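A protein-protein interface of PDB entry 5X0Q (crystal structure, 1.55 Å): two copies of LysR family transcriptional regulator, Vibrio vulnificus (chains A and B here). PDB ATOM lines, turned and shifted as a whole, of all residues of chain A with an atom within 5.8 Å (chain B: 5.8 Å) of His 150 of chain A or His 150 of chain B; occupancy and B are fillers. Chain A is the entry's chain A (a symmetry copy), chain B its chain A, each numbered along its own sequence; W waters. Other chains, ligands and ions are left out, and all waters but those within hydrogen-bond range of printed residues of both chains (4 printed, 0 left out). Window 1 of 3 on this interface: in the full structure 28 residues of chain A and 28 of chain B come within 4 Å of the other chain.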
ATOM      1  N   PRO A  24      -8.483  20.652 -23.724  1.00  0.00           N
ATOM      2  CA  PRO A  24      -8.760  21.508 -22.562  1.00  0.00           C
ATOM      3  C   PRO A  24      -9.648  22.708 -22.843  1.00  0.00           C
ATOM      4  O   PRO A  24     -10.293  23.196 -21.895  1.00  0.00           O
ATOM      5  CB  PRO A  24      -7.353  21.938 -22.109  1.00  0.00           C
ATOM      6  CG  PRO A  24      -6.445  20.882 -22.599  1.00  0.00           C
ATOM      7  CD  PRO A  24      -7.049  20.375 -23.888  1.00  0.00           C
ATOM      8  N   ALA A  27     -13.332  20.550 -23.153  1.00  0.00           N
ATOM      9  CA  ALA A  27     -13.782  19.553 -22.172  1.00  0.00           C
ATOM     10  C   ALA A  27     -14.490  20.142 -20.965  1.00  0.00           C
ATOM     11  O   ALA A  27     -15.546  19.604 -20.594  1.00  0.00           O
ATOM     12  CB  ALA A  27     -12.613  18.669 -21.690  1.00  0.00           C
ATOM     13  N   PRO A  28     -14.042  21.252 -20.363  1.00  0.00           N
ATOM     14  CA  PRO A  28     -14.736  21.753 -19.163  1.00  0.00           C
ATOM     15  C   PRO A  28     -16.125  22.249 -19.425  1.00  0.00           C
ATOM     16  O   PRO A  28     -16.865  22.504 -18.456  1.00  0.00           O
ATOM     17  CB  PRO A  28     -13.866  22.923 -18.721  1.00  0.00           C
ATOM     18  CG  PRO A  28     -12.460  22.648 -19.309  1.00  0.00           C
ATOM     19  CD  PRO A  28     -12.798  21.998 -20.658  1.00  0.00           C
ATOM     20  N   PHE A  29     -16.453  22.554 -20.679  1.00  0.00           N
ATOM     21  CA  PHE A  29     -17.679  23.257 -21.013  1.00  0.00           C
ATOM     22  C   PHE A  29     -18.659  22.252 -21.629  1.00  0.00           C
ATOM     23  O   PHE A  29     -19.604  21.802 -20.961  1.00  0.00           O
ATOM     24  CB  PHE A  29     -17.283  24.403 -21.952  1.00  0.00           C
ATOM     25  CG  PHE A  29     -16.047  25.183 -21.447  1.00  0.00           C
ATOM     26  CD1 PHE A  29     -16.076  25.837 -20.201  1.00  0.00           C
ATOM     27  CD2 PHE A  29     -14.883  25.217 -22.194  1.00  0.00           C
ATOM     28  CE1 PHE A  29     -14.982  26.526 -19.705  1.00  0.00           C
ATOM     29  CE2 PHE A  29     -13.750  25.902 -21.696  1.00  0.00           C
ATOM     30  CZ  PHE A  29     -13.808  26.554 -20.438  1.00  0.00           C
ATOM     31  N   LEU A  49     -13.362   9.489 -19.427  1.00  0.00           N
ATOM     32  CA  LEU A  49     -12.971  10.731 -20.076  1.00  0.00           C
ATOM     33  C   LEU A  49     -11.475  10.996 -19.903  1.00  0.00           C
ATOM     34  O   LEU A  49     -10.908  10.810 -18.810  1.00  0.00           O
ATOM     35  CB  LEU A  49     -13.743  11.930 -19.508  1.00  0.00           C
ATOM     36  CG  LEU A  49     -15.249  11.897 -19.766  1.00  0.00           C
ATOM     37  CD1 LEU A  49     -15.925  13.067 -18.998  1.00  0.00           C
ATOM     38  CD2 LEU A  49     -15.559  11.965 -21.271  1.00  0.00           C
ATOM     39  N   GLU A  51      -8.709  14.174 -20.761  1.00  0.00           N
ATOM     40  CA  GLU A  51      -8.454  15.531 -21.210  1.00  0.00           C
ATOM     41  C   GLU A  51      -6.972  15.677 -21.520  1.00  0.00           C
ATOM     42  O   GLU A  51      -6.115  15.366 -20.674  1.00  0.00           O
ATOM     43  CB  GLU A  51      -8.881  16.510 -20.127  1.00  0.00           C
ATOM     44  CG  GLU A  51      -8.666  17.958 -20.605  1.00  0.00           C
ATOM     45  CD  GLU A  51      -9.177  19.031 -19.627  1.00  0.00           C
ATOM     46  OE1 GLU A  51      -8.394  19.989 -19.420  1.00  0.00           O
ATOM     47  OE2 GLU A  51     -10.259  18.862 -19.010  1.00  0.00           O
ATOM     48  N   SER A 148      -3.159  28.014 -19.613  1.00  0.00           N
ATOM     49  CA  SER A 148      -4.507  27.479 -19.525  1.00  0.00           C
ATOM     50  C   SER A 148      -5.502  28.564 -19.871  1.00  0.00           C
ATOM     51  O   SER A 148      -5.237  29.770 -19.759  1.00  0.00           O
ATOM     52  CB  SER A 148      -4.840  26.902 -18.128  1.00  0.00           C
ATOM     53  OG  SER A 148      -4.964  27.988 -17.208  1.00  0.00           O
ATOM     54  N   LEU A 149      -6.696  28.121 -20.301  1.00  0.00           N
ATOM     55  CA  LEU A 149      -7.729  29.079 -20.612  1.00  0.00           C
ATOM     56  C   LEU A 149      -8.131  29.893 -19.367  1.00  0.00           C
ATOM     57  O   LEU A 149      -8.346  31.101 -19.443  1.00  0.00           O
ATOM     58  CB  LEU A 149      -8.911  28.311 -21.216  1.00  0.00           C
ATOM     59  CG  LEU A 149      -9.971  29.165 -21.894  1.00  0.00           C
ATOM     60  CD1 LEU A 149      -9.390  30.093 -22.939  1.00  0.00           C
ATOM     61  CD2 LEU A 149     -11.006  28.224 -22.527  1.00  0.00           C
ATOM     62  N   HIS A 150      -8.156  29.258 -18.185  1.00  0.00           N
ATOM     63  CA  HIS A 150      -8.523  29.991 -16.963  1.00  0.00           C
ATOM     64  C   HIS A 150      -7.524  31.093 -16.615  1.00  0.00           C
ATOM     65  O   HIS A 150      -7.925  32.198 -16.204  1.00  0.00           O
ATOM     66  CB  HIS A 150      -8.651  28.984 -15.805  1.00  0.00           C
ATOM     67  CG  HIS A 150      -9.606  27.896 -16.112  1.00  0.00           C
ATOM     68  ND1 HIS A 150      -9.236  26.737 -16.769  1.00  0.00           N
ATOM     69  CD2 HIS A 150     -10.941  27.819 -15.919  1.00  0.00           C
ATOM     70  CE1 HIS A 150     -10.312  25.992 -16.961  1.00  0.00           C
ATOM     71  NE2 HIS A 150     -11.353  26.617 -16.436  1.00  0.00           N
ATOM     72  N   THR A 151      -6.221  30.779 -16.671  1.00  0.00           N
ATOM     73  CA  THR A 151      -5.232  31.795 -16.296  1.00  0.00           C
ATOM     74  C   THR A 151      -5.071  32.829 -17.396  1.00  0.00           C
ATOM     75  O   THR A 151      -4.791  33.973 -17.099  1.00  0.00           O
ATOM     76  CB  THR A 151      -3.892  31.155 -15.952  1.00  0.00           C
ATOM     77  OG1 THR A 151      -3.442  30.314 -17.017  1.00  0.00           O
ATOM     78  CG2 THR A 151      -4.010  30.313 -14.613  1.00  0.00           C
ATOM     79  N   LEU A 152      -5.340  32.469 -18.660  1.00  0.00           N
ATOM     80  CA  LEU A 152      -5.405  33.477 -19.719  1.00  0.00           C
ATOM     81  C   LEU A 152      -6.469  34.527 -19.385  1.00  0.00           C
ATOM     82  O   LEU A 152      -6.233  35.748 -19.448  1.00  0.00           O
ATOM     83  CB  LEU A 152      -5.725  32.782 -21.071  1.00  0.00           C
ATOM     84  CG  LEU A 152      -5.991  33.643 -22.302  1.00  0.00           C
ATOM     85  CD1 LEU A 152      -4.833  34.600 -22.535  1.00  0.00           C
ATOM     86  CD2 LEU A 152      -6.277  32.789 -23.564  1.00  0.00           C
ATOM     87  N   VAL A 153      -7.683  34.067 -19.045  1.00  0.00           N
ATOM     88  CA  VAL A 153      -8.770  34.992 -18.744  1.00  0.00           C
ATOM     89  C   VAL A 153      -8.450  35.823 -17.507  1.00  0.00           C
ATOM     90  O   VAL A 153      -8.772  37.015 -17.440  1.00  0.00           O
ATOM     91  CB  VAL A 153     -10.083  34.215 -18.545  1.00  0.00           C
ATOM     92  CG1 VAL A 153     -11.176  35.123 -17.991  1.00  0.00           C
ATOM     93  CG2 VAL A 153     -10.547  33.579 -19.866  1.00  0.00           C
ATOM     94  N   GLN A 154      -7.821  35.197 -16.497  1.00  0.00           N
ATOM     95  CA  GLN A 154      -7.456  35.927 -15.286  1.00  0.00           C
ATOM     96  C   GLN A 154      -6.463  37.037 -15.591  1.00  0.00           C
ATOM     97  O   GLN A 154      -6.578  38.126 -15.032  1.00  0.00           O
ATOM     98  CB  GLN A 154      -6.879  34.965 -14.247  1.00  0.00           C
ATOM     99  CG  GLN A 154      -7.981  34.095 -13.613  1.00  0.00           C
ATOM    100  CD  GLN A 154      -7.434  32.755 -13.142  1.00  0.00           C
ATOM    101  OE1 GLN A 154      -6.247  32.477 -13.272  1.00  0.00           O
ATOM    102  NE2 GLN A 154      -8.334  31.895 -12.595  1.00  0.00           N
ATOM    103  N   MET A 155      -5.498  36.796 -16.499  1.00  0.00           N
ATOM    104  CA  MET A 155      -4.602  37.910 -16.872  1.00  0.00           C
ATOM    105  C   MET A 155      -5.384  39.050 -17.538  1.00  0.00           C
ATOM    106  O   MET A 155      -5.114  40.238 -17.280  1.00  0.00           O
ATOM    107  CB  MET A 155      -3.489  37.412 -17.801  1.00  0.00           C
ATOM    108  CG  MET A 155      -2.474  36.485 -17.070  1.00  0.00           C
ATOM    109  SD  MET A 155      -0.994  36.184 -18.008  1.00  0.00           S
ATOM    110  CE  MET A 155      -1.673  34.935 -19.134  1.00  0.00           C
ATOM    111  N   LEU A 174     -17.405  31.028 -17.568  1.00  0.00           N
ATOM    112  CA  LEU A 174     -15.983  31.261 -17.352  1.00  0.00           C
ATOM    113  C   LEU A 174     -15.717  32.685 -16.910  1.00  0.00           C
ATOM    114  O   LEU A 174     -14.810  32.923 -16.101  1.00  0.00           O
ATOM    115  CB  LEU A 174     -15.197  30.937 -18.634  1.00  0.00           C
ATOM    116  CG  LEU A 174     -13.683  31.087 -18.452  1.00  0.00           C
ATOM    117  CD1 LEU A 174     -13.132  30.106 -17.453  1.00  0.00           C
ATOM    118  CD2 LEU A 174     -12.965  30.850 -19.798  1.00  0.00           C
ATOM    119  N   GLN A 178     -15.604  38.165 -12.895  1.00  0.00           N
ATOM    120  CA  GLN A 178     -14.289  38.680 -13.258  1.00  0.00           C
ATOM    121  C   GLN A 178     -14.356  40.056 -13.906  1.00  0.00           C
ATOM    122  O   GLN A 178     -13.311  40.595 -14.321  1.00  0.00           O
ATOM    123  CB  GLN A 178     -13.556  37.685 -14.156  1.00  0.00           C
ATOM    124  CG  GLN A 178     -13.425  36.319 -13.444  1.00  0.00           C
ATOM    125  CD  GLN A 178     -12.309  35.468 -14.014  1.00  0.00           C
ATOM    126  OE1 GLN A 178     -12.548  34.470 -14.731  1.00  0.00           O
ATOM    127  NE2 GLN A 178     -11.094  35.859 -13.727  1.00  0.00           N
ATOM    128  N   PRO B  24      -3.179  23.158 -11.376  1.00  0.00           N
ATOM    129  CA  PRO B  24      -4.503  23.101 -12.013  1.00  0.00           C
ATOM    130  C   PRO B  24      -5.670  22.927 -11.057  1.00  0.00           C
ATOM    131  O   PRO B  24      -6.793  23.322 -11.424  1.00  0.00           O
ATOM    132  CB  PRO B  24      -4.371  21.904 -12.970  1.00  0.00           C
ATOM    133  CG  PRO B  24      -2.927  21.785 -13.252  1.00  0.00           C
ATOM    134  CD  PRO B  24      -2.216  22.239 -11.998  1.00  0.00           C
ATOM    135  N   ALA B  27      -5.678  26.929  -9.535  1.00  0.00           N
ATOM    136  CA  ALA B  27      -5.632  28.128 -10.384  1.00  0.00           C
ATOM    137  C   ALA B  27      -6.985  28.568 -10.914  1.00  0.00           C
ATOM    138  O   ALA B  27      -7.269  29.775 -10.845  1.00  0.00           O
ATOM    139  CB  ALA B  27      -4.660  27.943 -11.568  1.00  0.00           C
ATOM    140  N   PRO B  28      -7.881  27.681 -11.369  1.00  0.00           N
ATOM    141  CA  PRO B  28      -9.158  28.165 -11.922  1.00  0.00           C
ATOM    142  C   PRO B  28     -10.055  28.810 -10.909  1.00  0.00           C
ATOM    143  O   PRO B  28     -11.061  29.427 -11.305  1.00  0.00           O
ATOM    144  CB  PRO B  28      -9.821  26.892 -12.432  1.00  0.00           C
ATOM    145  CG  PRO B  28      -8.668  25.888 -12.684  1.00  0.00           C
ATOM    146  CD  PRO B  28      -7.697  26.223 -11.543  1.00  0.00           C
ATOM    147  N   PHE B  29      -9.827  28.555  -9.623  1.00  0.00           N
ATOM    148  CA  PHE B  29     -10.764  28.932  -8.579  1.00  0.00           C
ATOM    149  C   PHE B  29     -10.191  30.140  -7.829  1.00  0.00           C
ATOM    150  O   PHE B  29     -10.631  31.282  -8.042  1.00  0.00           O
ATOM    151  CB  PHE B  29     -10.966  27.689  -7.703  1.00  0.00           C
ATOM    152  CG  PHE B  29     -11.198  26.408  -8.538  1.00  0.00           C
ATOM    153  CD1 PHE B  29     -12.296  26.317  -9.414  1.00  0.00           C
ATOM    154  CD2 PHE B  29     -10.311  25.349  -8.464  1.00  0.00           C
ATOM    155  CE1 PHE B  29     -12.524  25.195 -10.194  1.00  0.00           C
ATOM    156  CE2 PHE B  29     -10.519  24.203  -9.266  1.00  0.00           C
ATOM    157  CZ  PHE B  29     -11.634  24.137 -10.139  1.00  0.00           C
ATOM    158  N   LEU B  49       0.645  34.848 -15.326  1.00  0.00           N
ATOM    159  CA  LEU B  49       0.230  33.618 -14.669  1.00  0.00           C
ATOM    160  C   LEU B  49       0.660  32.391 -15.475  1.00  0.00           C
ATOM    161  O   LEU B  49       0.537  32.356 -16.713  1.00  0.00           O
ATOM    162  CB  LEU B  49      -1.293  33.565 -14.484  1.00  0.00           C
ATOM    163  CG  LEU B  49      -1.857  34.632 -13.546  1.00  0.00           C
ATOM    164  CD1 LEU B  49      -3.410  34.574 -13.583  1.00  0.00           C
ATOM    165  CD2 LEU B  49      -1.326  34.453 -12.115  1.00  0.00           C
ATOM    166  N   GLU B  51       0.048  28.138 -15.323  1.00  0.00           N
ATOM    167  CA  GLU B  51      -0.613  26.983 -14.741  1.00  0.00           C
ATOM    168  C   GLU B  51       0.132  25.726 -15.162  1.00  0.00           C
ATOM    169  O   GLU B  51       0.357  25.497 -16.363  1.00  0.00           O
ATOM    170  CB  GLU B  51      -2.060  26.941 -15.209  1.00  0.00           C
ATOM    171  CG  GLU B  51      -2.792  25.751 -14.562  1.00  0.00           C
ATOM    172  CD  GLU B  51      -4.297  25.684 -14.878  1.00  0.00           C
ATOM    173  OE1 GLU B  51      -4.731  24.552 -15.199  1.00  0.00           O
ATOM    174  OE2 GLU B  51      -4.983  26.736 -14.914  1.00  0.00           O
ATOM    175  N   SER B 148      -8.062  15.577 -15.631  1.00  0.00           N
ATOM    176  CA  SER B 148      -8.350  16.928 -15.182  1.00  0.00           C
ATOM    177  C   SER B 148      -9.452  16.890 -14.148  1.00  0.00           C
ATOM    178  O   SER B 148     -10.268  15.959 -14.079  1.00  0.00           O
ATOM    179  CB  SER B 148      -8.759  17.875 -16.335  1.00  0.00           C
ATOM    180  OG  SER B 148     -10.061  17.502 -16.787  1.00  0.00           O
ATOM    181  N   LEU B 149      -9.484  17.945 -13.315  1.00  0.00           N
ATOM    182  CA  LEU B 149     -10.528  18.025 -12.323  1.00  0.00           C
ATOM    183  C   LEU B 149     -11.920  18.105 -12.979  1.00  0.00           C
ATOM    184  O   LEU B 149     -12.874  17.481 -12.519  1.00  0.00           O
ATOM    185  CB  LEU B 149     -10.230  19.234 -11.428  1.00  0.00           C
ATOM    186  CG  LEU B 149     -11.033  19.310 -10.139  1.00  0.00           C
ATOM    187  CD1 LEU B 149     -10.936  18.043  -9.317  1.00  0.00           C
ATOM    188  CD2 LEU B 149     -10.525  20.514  -9.333  1.00  0.00           C
ATOM    189  N   HIS B 150     -12.036  18.811 -14.115  1.00  0.00           N
ATOM    190  CA  HIS B 150     -13.341  18.913 -14.788  1.00  0.00           C
ATOM    191  C   HIS B 150     -13.846  17.564 -15.298  1.00  0.00           C
ATOM    192  O   HIS B 150     -15.048  17.260 -15.183  1.00  0.00           O
ATOM    193  CB  HIS B 150     -13.220  19.924 -15.944  1.00  0.00           C
ATOM    194  CG  HIS B 150     -12.723  21.241 -15.487  1.00  0.00           C
ATOM    195  ND1 HIS B 150     -11.378  21.543 -15.392  1.00  0.00           N
ATOM    196  CD2 HIS B 150     -13.393  22.319 -15.022  1.00  0.00           C
ATOM    197  CE1 HIS B 150     -11.246  22.759 -14.891  1.00  0.00           C
ATOM    198  NE2 HIS B 150     -12.453  23.257 -14.678  1.00  0.00           N
ATOM    199  N   THR B 151     -12.971  16.791 -15.957  1.00  0.00           N
ATOM    200  CA  THR B 151     -13.431  15.511 -16.506  1.00  0.00           C
ATOM    201  C   THR B 151     -13.584  14.473 -15.408  1.00  0.00           C
ATOM    202  O   THR B 151     -14.436  13.614 -15.517  1.00  0.00           O
ATOM    203  CB  THR B 151     -12.492  15.013 -17.598  1.00  0.00           C
ATOM    204  OG1 THR B 151     -11.144  14.956 -17.122  1.00  0.00           O
ATOM    205  CG2 THR B 151     -12.575  15.956 -18.871  1.00  0.00           C
ATOM    206  N   LEU B 152     -12.835  14.593 -14.302  1.00  0.00           N
ATOM    207  CA  LEU B 152     -13.094  13.747 -13.136  1.00  0.00           C
ATOM    208  C   LEU B 152     -14.533  13.947 -12.649  1.00  0.00           C
ATOM    209  O   LEU B 152     -15.289  12.985 -12.415  1.00  0.00           O
ATOM    210  CB  LEU B 152     -12.081  14.096 -12.012  1.00  0.00           C
ATOM    211  CG  LEU B 152     -12.245  13.450 -10.640  1.00  0.00           C
ATOM    212  CD1 LEU B 152     -12.289  11.936 -10.772  1.00  0.00           C
ATOM    213  CD2 LEU B 152     -11.142  13.896  -9.646  1.00  0.00           C
ATOM    214  N   VAL B 153     -14.935  15.213 -12.458  1.00  0.00           N
ATOM    215  CA  VAL B 153     -16.276  15.501 -11.963  1.00  0.00           C
ATOM    216  C   VAL B 153     -17.334  15.038 -12.957  1.00  0.00           C
ATOM    217  O   VAL B 153     -18.396  14.537 -12.571  1.00  0.00           O
ATOM    218  CB  VAL B 153     -16.422  17.006 -11.683  1.00  0.00           C
ATOM    219  CG1 VAL B 153     -17.877  17.370 -11.401  1.00  0.00           C
ATOM    220  CG2 VAL B 153     -15.536  17.431 -10.501  1.00  0.00           C
ATOM    221  N   GLN B 154     -17.064  15.215 -14.262  1.00  0.00           N
ATOM    222  CA  GLN B 154     -18.014  14.777 -15.282  1.00  0.00           C
ATOM    223  C   GLN B 154     -18.213  13.271 -15.237  1.00  0.00           C
ATOM    224  O   GLN B 154     -19.339  12.801 -15.389  1.00  0.00           O
ATOM    225  CB  GLN B 154     -17.535  15.212 -16.668  1.00  0.00           C
ATOM    226  CG  GLN B 154     -17.724  16.726 -16.878  1.00  0.00           C
ATOM    227  CD  GLN B 154     -16.706  17.286 -17.862  1.00  0.00           C
ATOM    228  OE1 GLN B 154     -15.876  16.557 -18.394  1.00  0.00           O
ATOM    229  NE2 GLN B 154     -16.765  18.624 -18.094  1.00  0.00           N
ATOM    230  N   MET B 155     -17.139  12.494 -14.999  1.00  0.00           N
ATOM    231  CA  MET B 155     -17.353  11.040 -14.850  1.00  0.00           C
ATOM    232  C   MET B 155     -18.241  10.733 -13.635  1.00  0.00           C
ATOM    233  O   MET B 155     -19.112   9.845 -13.696  1.00  0.00           O
ATOM    234  CB  MET B 155     -16.010  10.312 -14.726  1.00  0.00           C
ATOM    235  CG  MET B 155     -15.201  10.327 -16.056  1.00  0.00           C
ATOM    236  SD  MET B 155     -13.824   9.202 -16.055  1.00  0.00           S
ATOM    237  CE  MET B 155     -12.682  10.220 -15.082  1.00  0.00           C
ATOM    238  N   LEU B 174     -18.019  24.646  -9.733  1.00  0.00           N
ATOM    239  CA  LEU B 174     -17.621  23.505 -10.546  1.00  0.00           C
ATOM    240  C   LEU B 174     -18.758  22.515 -10.703  1.00  0.00           C
ATOM    241  O   LEU B 174     -18.894  21.892 -11.764  1.00  0.00           O
ATOM    242  CB  LEU B 174     -16.391  22.822  -9.926  1.00  0.00           C
ATOM    243  CG  LEU B 174     -15.871  21.657 -10.776  1.00  0.00           C
ATOM    244  CD1 LEU B 174     -15.372  22.113 -12.119  1.00  0.00           C
ATOM    245  CD2 LEU B 174     -14.706  20.953 -10.048  1.00  0.00           C
ATOM    246  N   GLN B 178     -24.679  19.935 -12.811  1.00  0.00           N
ATOM    247  CA  GLN B 178     -24.258  18.553 -13.017  1.00  0.00           C
ATOM    248  C   GLN B 178     -24.990  17.576 -12.108  1.00  0.00           C
ATOM    249  O   GLN B 178     -24.690  16.365 -12.134  1.00  0.00           O
ATOM    250  CB  GLN B 178     -22.745  18.427 -12.857  1.00  0.00           C
ATOM    251  CG  GLN B 178     -22.022  19.366 -13.850  1.00  0.00           C
ATOM    252  CD  GLN B 178     -20.591  18.946 -14.115  1.00  0.00           C
ATOM    253  OE1 GLN B 178     -19.623  19.580 -13.638  1.00  0.00           O
ATOM    254  NE2 GLN B 178     -20.442  17.873 -14.850  1.00  0.00           N
HETATM  255  O   HOH W   1     -10.329  12.392 -16.698  1.00  0.00           O
HETATM  256  O   HOH W   2      -7.096  24.727 -16.270  1.00  0.00           O
HETATM  257  O   HOH W   3      -1.374  31.439 -18.388  1.00  0.00           O
HETATM  258  O   HOH W   4      -9.126  21.360 -17.333  1.00  0.00           O
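OG of Ser 148 of chain A is in hydrogen-bond range of OE2 of Glu 51 of chain B, 2.6 Å away. The side-chain amide nitrogen (NE2) of Gln 154 of chain B is in hydrogen-bond range of the backbone carbonyl oxygen (O) of Ala 27 of chain A (2.9 Å). SD of Met 155 of chain B sits at hydrogen-bond distance from N of Leu 49 of chain A (3.4 Å). OG of Ser 148 of chain B lies within hydrogen-bond range of OE2 of Glu 51 of chain A, at 2.6 Å. The backbone NH (N) of Leu 49 of chain B sits at hydrogen-bond distance from the side-chain sulfur (SD) of Met 155 of chain A, 3.4 Å away. O of Ala 27 of chain B is in hydrogen-bond range of NE2 of Gln 154 of chain A (2.9 Å).
The side-chain hydroxyl (OG) of Ser 148 of chain A is in hydrogen-bond range of the side-chain hydroxyl (OG1) of Thr 151 of chain A. The backbone carbonyl oxygen (O) of His 150 of chain A lies close to the side-chain amide oxygen (OE1) of Gln 154 of chain A (3.4 Å). OG of Ser 148 of chain B sits at hydrogen-bond distance from OG1 of Thr 151 of chain B, 2.8 Å away. O of His 150 of chain B lies close to OE1 of Gln 154 of chain B.
Among the printed residues, merely in contact across the chains: Gln 154 of chain A with Leu 49 of chain B (3.5 Å), Leu 49 of chain A with Gln 154 of chain B (3.5 Å), Glu 51 of chain A with Thr 151 of chain B (3.7 Å), Thr 151 of chain A with Glu 51 of chain B (3.7 Å), Pro 28 of chain A with His 150 of chain B (3.8 Å), His 150 of chain A with Pro 28 of chain B (3.8 Å), Thr 151 of chain A with Leu 49 of chain B (3.8 Å), Leu 49 of chain A with Thr 151 of chain B (3.8 Å), Gln 154 of chain A with Pro 28 of chain B (3.9 Å), Pro 28 of chain A with Gln 154 of chain B (3.9 Å), Ala 27 of chain A with Thr 151 of chain B (3.9 Å), Thr 151 of chain A with Ala 27 of chain B (3.9 Å) and His 150 of chain A with His 150 of chain B (3.9 Å).
His 150 of chain B touches just these residues of chain A: Pro 28 and His 150. Of the printed residues of chain A, Pro 28 of chain B touches His 150 and Gln 154. Of the printed residues of chain B, Pro 28 of chain A touches His 150 and Gln 154. Leu 152 of chain B touches none of the printed residues of chain A. The nearest printed residue of chain B that does not touch Gln 154 of chain A is Phe 29 of chain B (4.7 Å).
Printed residues of chain A that touch a printed residue of chain B: Ala 27, Pro 28, Leu 49, Glu 51, Ser 148, His 150, Thr 151, Gln 154 and Met 155. Among the printed residues, 19 pairs touch across the chains. Among the printed residues, no Asp or Glu carboxylate lies within 4 Å of a Lys or Arg side-chain nitrogen of the other chain.
Pro 28 of chain A touches Gln 154 of chain B, and with the chains exchanged Gln 154 of chain A touches Pro 28 of chain B. Leu 49 of chain A touches Thr 151 of chain B, and with the chains exchanged Thr 151 of chain A touches Leu 49 of chain B. Leu 49 of chain A touches Met 155 of chain B, and with the chains exchanged Met 155 of chain A touches Leu 49 of chain B. His 150 of chain A touches its own counterpart, His 150 of chain B. Of the 19 pairs that touch across the chains among the printed residues, 19 have their exchanged pair printed and touching as well.
Water W2 bridges OE1 of Glu 51 of chain B (2.6 Å) and ND1 of His 150 of chain A (3.0 Å). Water W4 bridges the side-chain carboxylate (OE1) of Glu 51 of chain A and a ring nitrogen (ND1) of His 150 of chain B. Water W3 lies within hydrogen-bond range of O of Leu 49 of chain B (2.7 Å) and OG1 of Thr 151 of chain A (2.7 Å). Water W1 bridges O of Leu 49 of chain A and OG1 of Thr 151 of chain B.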
